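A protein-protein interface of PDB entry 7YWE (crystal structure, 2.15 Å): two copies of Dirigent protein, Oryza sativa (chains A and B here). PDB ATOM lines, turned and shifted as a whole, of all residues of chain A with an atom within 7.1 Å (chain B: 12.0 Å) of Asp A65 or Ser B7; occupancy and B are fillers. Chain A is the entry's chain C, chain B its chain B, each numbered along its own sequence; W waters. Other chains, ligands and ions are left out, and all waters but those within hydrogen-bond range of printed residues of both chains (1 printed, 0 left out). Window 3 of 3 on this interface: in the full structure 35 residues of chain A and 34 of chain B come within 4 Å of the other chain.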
ATOM      1  N   PHE A  25      -8.932   3.456  23.467  1.00  0.00           N
ATOM      2  CA  PHE A  25     -10.300   3.111  23.829  1.00  0.00           C
ATOM      3  C   PHE A  25     -10.637   1.717  23.319  1.00  0.00           C
ATOM      4  O   PHE A  25     -10.303   1.361  22.185  1.00  0.00           O
ATOM      5  CB  PHE A  25     -11.298   4.109  23.238  1.00  0.00           C
ATOM      6  CG  PHE A  25     -11.223   5.481  23.834  1.00  0.00           C
ATOM      7  CD1 PHE A  25     -10.312   6.409  23.359  1.00  0.00           C
ATOM      8  CD2 PHE A  25     -12.087   5.854  24.851  1.00  0.00           C
ATOM      9  CE1 PHE A  25     -10.252   7.679  23.900  1.00  0.00           C
ATOM     10  CE2 PHE A  25     -12.032   7.121  25.394  1.00  0.00           C
ATOM     11  CZ  PHE A  25     -11.113   8.035  24.917  1.00  0.00           C
ATOM     12  N   THR A  26     -11.318   0.936  24.155  1.00  0.00           N
ATOM     13  CA  THR A  26     -11.781  -0.385  23.760  1.00  0.00           C
ATOM     14  C   THR A  26     -13.212  -0.588  24.231  1.00  0.00           C
ATOM     15  O   THR A  26     -13.648   0.007  25.221  1.00  0.00           O
ATOM     16  CB  THR A  26     -10.890  -1.503  24.322  1.00  0.00           C
ATOM     17  OG1 THR A  26     -10.666  -1.283  25.720  1.00  0.00           O
ATOM     18  CG2 THR A  26      -9.557  -1.550  23.590  1.00  0.00           C
ATOM     19  N   LYS A  27     -13.939  -1.435  23.499  1.00  0.00           N
ATOM     20  CA  LYS A  27     -15.300  -1.840  23.854  1.00  0.00           C
ATOM     21  C   LYS A  27     -16.252  -0.646  23.919  1.00  0.00           C
ATOM     22  O   LYS A  27     -17.053  -0.517  24.847  1.00  0.00           O
ATOM     23  CB  LYS A  27     -15.319  -2.629  25.167  1.00  0.00           C
ATOM     24  CG  LYS A  27     -14.595  -3.965  25.083  1.00  0.00           C
ATOM     25  CD  LYS A  27     -14.781  -4.793  26.347  1.00  0.00           C
ATOM     26  CE  LYS A  27     -14.098  -6.146  26.216  1.00  0.00           C
ATOM     27  NZ  LYS A  27     -14.320  -7.012  27.407  1.00  0.00           N
ATOM     28  N   LEU A  28     -16.161   0.233  22.926  1.00  0.00           N
ATOM     29  CA  LEU A  28     -17.162   1.265  22.694  1.00  0.00           C
ATOM     30  C   LEU A  28     -18.133   0.765  21.632  1.00  0.00           C
ATOM     31  O   LEU A  28     -17.709   0.217  20.610  1.00  0.00           O
ATOM     32  CB  LEU A  28     -16.513   2.577  22.248  1.00  0.00           C
ATOM     33  CG  LEU A  28     -15.730   3.373  23.294  1.00  0.00           C
ATOM     34  CD1 LEU A  28     -14.902   4.454  22.626  1.00  0.00           C
ATOM     35  CD2 LEU A  28     -16.672   3.984  24.319  1.00  0.00           C
ATOM     36  N   TYR A  29     -19.429   0.948  21.871  1.00  0.00           N
ATOM     37  CA  TYR A  29     -20.465   0.380  21.014  1.00  0.00           C
ATOM     38  C   TYR A  29     -21.354   1.495  20.477  1.00  0.00           C
ATOM     39  O   TYR A  29     -22.113   2.113  21.232  1.00  0.00           O
ATOM     40  CB  TYR A  29     -21.275  -0.667  21.776  1.00  0.00           C
ATOM     41  CG  TYR A  29     -20.430  -1.839  22.223  1.00  0.00           C
ATOM     42  CD1 TYR A  29     -19.787  -1.827  23.455  1.00  0.00           C
ATOM     43  CD2 TYR A  29     -20.258  -2.948  21.402  1.00  0.00           C
ATOM     44  CE1 TYR A  29     -19.005  -2.892  23.863  1.00  0.00           C
ATOM     45  CE2 TYR A  29     -19.478  -4.016  21.801  1.00  0.00           C
ATOM     46  CZ  TYR A  29     -18.855  -3.982  23.032  1.00  0.00           C
ATOM     47  OH  TYR A  29     -18.079  -5.046  23.429  1.00  0.00           O
ATOM     48  N   VAL A  63     -23.306   6.303  21.532  1.00  0.00           N
ATOM     49  CA  VAL A  63     -22.231   5.372  21.857  1.00  0.00           C
ATOM     50  C   VAL A  63     -22.389   4.950  23.311  1.00  0.00           C
ATOM     51  O   VAL A  63     -22.508   5.800  24.201  1.00  0.00           O
ATOM     52  CB  VAL A  63     -20.843   5.990  21.611  1.00  0.00           C
ATOM     53  CG1 VAL A  63     -19.752   4.971  21.901  1.00  0.00           C
ATOM     54  CG2 VAL A  63     -20.734   6.496  20.177  1.00  0.00           C
ATOM     55  N   TYR A  64     -22.393   3.640  23.546  1.00  0.00           N
ATOM     56  CA  TYR A  64     -22.577   3.075  24.873  1.00  0.00           C
ATOM     57  C   TYR A  64     -21.323   2.326  25.303  1.00  0.00           C
ATOM     58  O   TYR A  64     -20.454   2.003  24.488  1.00  0.00           O
ATOM     59  CB  TYR A  64     -23.792   2.138  24.912  1.00  0.00           C
ATOM     60  CG  TYR A  64     -25.113   2.858  24.785  1.00  0.00           C
ATOM     61  CD1 TYR A  64     -25.612   3.222  23.542  1.00  0.00           C
ATOM     62  CD2 TYR A  64     -25.861   3.177  25.911  1.00  0.00           C
ATOM     63  CE1 TYR A  64     -26.817   3.884  23.422  1.00  0.00           C
ATOM     64  CE2 TYR A  64     -27.069   3.839  25.802  1.00  0.00           C
ATOM     65  CZ  TYR A  64     -27.542   4.190  24.554  1.00  0.00           C
ATOM     66  OH  TYR A  64     -28.744   4.849  24.439  1.00  0.00           O
ATOM     67  N   ASP A  65     -21.246   2.045  26.602  1.00  0.00           N
ATOM     68  CA  ASP A  65     -20.089   1.382  27.189  1.00  0.00           C
ATOM     69  C   ASP A  65     -20.199  -0.138  27.176  1.00  0.00           C
ATOM     70  O   ASP A  65     -19.310  -0.811  27.710  1.00  0.00           O
ATOM     71  CB  ASP A  65     -19.873   1.874  28.627  1.00  0.00           C
ATOM     72  CG  ASP A  65     -21.093   1.664  29.512  1.00  0.00           C
ATOM     73  OD1 ASP A  65     -22.135   1.196  29.006  1.00  0.00           O
ATOM     74  OD2 ASP A  65     -21.008   1.971  30.719  1.00  0.00           O
ATOM     75  N   GLY A  66     -21.254  -0.689  26.588  1.00  0.00           N
ATOM     76  CA  GLY A  66     -21.413  -2.128  26.557  1.00  0.00           C
ATOM     77  C   GLY A  66     -22.698  -2.510  25.856  1.00  0.00           C
ATOM     78  O   GLY A  66     -23.411  -1.660  25.318  1.00  0.00           O
ATOM     79  N   ILE A  67     -22.981  -3.810  25.867  1.00  0.00           N
ATOM     80  CA  ILE A  67     -24.197  -4.359  25.281  1.00  0.00           C
ATOM     81  C   ILE A  67     -25.142  -4.762  26.404  1.00  0.00           C
ATOM     82  O   ILE A  67     -24.716  -5.089  27.518  1.00  0.00           O
ATOM     83  CB  ILE A  67     -23.905  -5.558  24.356  1.00  0.00           C
ATOM     84  CG1 ILE A  67     -23.253  -6.697  25.143  1.00  0.00           C
ATOM     85  CG2 ILE A  67     -23.023  -5.135  23.195  1.00  0.00           C
ATOM     86  CD1 ILE A  67     -22.949  -7.922  24.309  1.00  0.00           C
ATOM     87  N   ASP A  70     -28.176  -2.813  30.650  1.00  0.00           N
ATOM     88  CA  ASP A  70     -27.408  -2.137  31.686  1.00  0.00           C
ATOM     89  C   ASP A  70     -26.359  -1.186  31.120  1.00  0.00           C
ATOM     90  O   ASP A  70     -25.571  -0.627  31.888  1.00  0.00           O
ATOM     91  CB  ASP A  70     -26.739  -3.168  32.599  1.00  0.00           C
ATOM     92  CG  ASP A  70     -25.991  -4.240  31.824  1.00  0.00           C
ATOM     93  OD1 ASP A  70     -25.902  -4.126  30.583  1.00  0.00           O
ATOM     94  OD2 ASP A  70     -25.499  -5.199  32.458  1.00  0.00           O
ATOM     95  N   ALA A  71     -26.333  -0.992  29.805  1.00  0.00           N
ATOM     96  CA  ALA A  71     -25.328  -0.137  29.191  1.00  0.00           C
ATOM     97  C   ALA A  71     -25.646   1.334  29.434  1.00  0.00           C
ATOM     98  O   ALA A  71     -26.809   1.744  29.437  1.00  0.00           O
ATOM     99  CB  ALA A  71     -25.238  -0.411  27.691  1.00  0.00           C
ATOM    100  N   LYS A  72     -24.598   2.127  29.633  1.00  0.00           N
ATOM    101  CA  LYS A  72     -24.718   3.558  29.865  1.00  0.00           C
ATOM    102  C   LYS A  72     -24.227   4.322  28.643  1.00  0.00           C
ATOM    103  O   LYS A  72     -23.230   3.943  28.020  1.00  0.00           O
ATOM    104  CB  LYS A  72     -23.920   3.982  31.103  1.00  0.00           C
ATOM    105  CG  LYS A  72     -23.964   5.472  31.395  1.00  0.00           C
ATOM    106  CD  LYS A  72     -23.036   5.837  32.542  1.00  0.00           C
ATOM    107  CE  LYS A  72     -22.985   7.342  32.751  1.00  0.00           C
ATOM    108  NZ  LYS A  72     -22.034   7.721  33.832  1.00  0.00           N
ATOM    109  N   LEU A  73     -24.938   5.392  28.297  1.00  0.00           N
ATOM    110  CA  LEU A  73     -24.522   6.241  27.191  1.00  0.00           C
ATOM    111  C   LEU A  73     -23.324   7.084  27.607  1.00  0.00           C
ATOM    112  O   LEU A  73     -23.374   7.799  28.612  1.00  0.00           O
ATOM    113  CB  LEU A  73     -25.679   7.133  26.746  1.00  0.00           C
ATOM    114  CG  LEU A  73     -25.413   8.119  25.608  1.00  0.00           C
ATOM    115  CD1 LEU A  73     -26.584   8.130  24.645  1.00  0.00           C
ATOM    116  CD2 LEU A  73     -25.167   9.513  26.159  1.00  0.00           C
ATOM    117  N   VAL A  74     -22.245   7.003  26.832  1.00  0.00           N
ATOM    118  CA  VAL A  74     -21.014   7.706  27.166  1.00  0.00           C
ATOM    119  C   VAL A  74     -20.624   8.763  26.142  1.00  0.00           C
ATOM    120  O   VAL A  74     -19.887   9.698  26.496  1.00  0.00           O
ATOM    121  CB  VAL A  74     -19.849   6.715  27.374  1.00  0.00           C
ATOM    122  CG1 VAL A  74     -20.127   5.810  28.569  1.00  0.00           C
ATOM    123  CG2 VAL A  74     -19.619   5.890  26.119  1.00  0.00           C
ATOM    124  N   ALA A  75     -21.079   8.674  24.894  1.00  0.00           N
ATOM    125  CA  ALA A  75     -20.655   9.635  23.886  1.00  0.00           C
ATOM    126  C   ALA A  75     -21.652   9.652  22.737  1.00  0.00           C
ATOM    127  O   ALA A  75     -22.460   8.734  22.573  1.00  0.00           O
ATOM    128  CB  ALA A  75     -19.248   9.316  23.370  1.00  0.00           C
ATOM    129  N   SER B   7     -16.820   0.336  28.853  1.00  0.00           N
ATOM    130  CA  SER B   7     -15.664   0.603  28.006  1.00  0.00           C
ATOM    131  C   SER B   7     -14.387   0.699  28.836  1.00  0.00           C
ATOM    132  O   SER B   7     -14.431   0.652  30.066  1.00  0.00           O
ATOM    133  CB  SER B   7     -15.876   1.888  27.203  1.00  0.00           C
ATOM    134  OG  SER B   7     -16.075   3.001  28.056  1.00  0.00           O
ATOM    135  N   LYS B   8     -13.251   0.837  28.156  1.00  0.00           N
ATOM    136  CA  LYS B   8     -11.948   0.863  28.805  1.00  0.00           C
ATOM    137  C   LYS B   8     -11.038   1.836  28.073  1.00  0.00           C
ATOM    138  O   LYS B   8     -10.874   1.736  26.853  1.00  0.00           O
ATOM    139  CB  LYS B   8     -11.321  -0.537  28.829  1.00  0.00           C
ATOM    140  CG  LYS B   8      -9.903  -0.590  29.373  1.00  0.00           C
ATOM    141  CD  LYS B   8      -9.346  -2.003  29.281  1.00  0.00           C
ATOM    142  CE  LYS B   8      -7.899  -2.064  29.729  1.00  0.00           C
ATOM    143  NZ  LYS B   8      -7.332  -3.434  29.598  1.00  0.00           N
ATOM    144  N   LEU B   9     -10.447   2.769  28.817  1.00  0.00           N
ATOM    145  CA  LEU B   9      -9.548   3.779  28.269  1.00  0.00           C
ATOM    146  C   LEU B   9      -8.189   3.641  28.945  1.00  0.00           C
ATOM    147  O   LEU B   9      -8.068   3.867  30.153  1.00  0.00           O
ATOM    148  CB  LEU B   9     -10.114   5.185  28.466  1.00  0.00           C
ATOM    149  CG  LEU B   9      -9.145   6.353  28.254  1.00  0.00           C
ATOM    150  CD1 LEU B   9      -8.618   6.388  26.825  1.00  0.00           C
ATOM    151  CD2 LEU B   9      -9.814   7.669  28.615  1.00  0.00           C
ATOM    152  N   GLN B  10      -7.175   3.273  28.169  1.00  0.00           N
ATOM    153  CA  GLN B  10      -5.807   3.173  28.655  1.00  0.00           C
ATOM    154  C   GLN B  10      -4.987   4.357  28.163  1.00  0.00           C
ATOM    155  O   GLN B  10      -5.084   4.752  26.997  1.00  0.00           O
ATOM    156  CB  GLN B  10      -5.151   1.869  28.198  1.00  0.00           C
ATOM    157  CG  GLN B  10      -5.611   0.638  28.950  1.00  0.00           C
ATOM    158  CD  GLN B  10      -4.771  -0.582  28.627  1.00  0.00           C
ATOM    159  OE1 GLN B  10      -4.723  -1.031  27.481  1.00  0.00           O
ATOM    160  NE2 GLN B  10      -4.093  -1.117  29.636  1.00  0.00           N
ATOM    161  N   ILE B  11      -4.176   4.917  29.057  1.00  0.00           N
ATOM    162  CA  ILE B  11      -3.318   6.055  28.749  1.00  0.00           C
ATOM    163  C   ILE B  11      -1.880   5.648  29.039  1.00  0.00           C
ATOM    164  O   ILE B  11      -1.553   5.267  30.170  1.00  0.00           O
ATOM    165  CB  ILE B  11      -3.715   7.303  29.553  1.00  0.00           C
ATOM    166  CG1 ILE B  11      -5.203   7.608  29.358  1.00  0.00           C
ATOM    167  CG2 ILE B  11      -2.875   8.496  29.132  1.00  0.00           C
ATOM    168  CD1 ILE B  11      -5.691   8.813  30.134  1.00  0.00           C
HETATM  169  O   HOH W   1      -7.609  -0.511  25.972  1.00  0.00           O
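The backbone carbonyl oxygen of Lys B8 lies within hydrogen-bond range of the backbone NH of Thr A26 (2.8 Å).
The backbone carbonyl oxygen (O) of Asp A65 lies within hydrogen-bond range of the backbone NH (N) of Ser B7 (3.0 Å).
The side-chain carboxylate (OD1) of Asp A65 sits at hydrogen-bond distance from the backbone NH (N) of Lys A72 (2.7 Å).
Among the printed residues, pairs that only touch across the chains: Phe A25 with Lys B8 (3.4 Å), Phe A25 with Leu B9 (3.5 Å), Thr A26 with Ser B7 (3.5 Å), Lys A27 with Ser B7 (3.6 Å) and Leu A28 with Ser B7 (3.7 Å).
Of chain B, only Ser B7 (3.0 Å) comes within 4 Å of Asp A65.
Of chain A, only Thr A26 (3.5 Å), Lys A27 (3.6 Å), Leu A28 (3.7 Å) and Asp A65 (3.0 Å) come within 4 Å of Ser B7.
Of chain B, only Ser B7 and Lys B8 come within 4 Å of Thr A26.
Of chain B, only Ser B7 (3.6 Å) comes within 4 Å of Lys A27.
Of chain B, only Ser B7 (3.7 Å) comes within 4 Å of Leu A28.
No residue of chain B comes within 4 Å of Tyr A29.
No residue of chain B comes within 4 Å of Val A63.
No residue of chain B comes within 4 Å of Gly A66.
No residue of chain B comes within 4 Å of Val A74.
Of the printed residues of chain A, Leu B9 touches Phe A25 (3.5 Å).
Of the printed residues of chain B, Phe A25 touches Lys B8 and Leu B9.
Asp A70 touches none of the printed residues of chain B.
Hydrophobic or aromatic side chains of chain A within 4 Å of the printed part of chain B: Phe A25 and Leu A28.
Among the printed residues, no Asp or Glu carboxylate lies within 4 Å of a Lys or Arg side-chain nitrogen of the other chain.
No position is printed for both chains.
Water W1 lies within hydrogen-bond range of OG1 of Thr A26 and OE1 of Gln B10.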
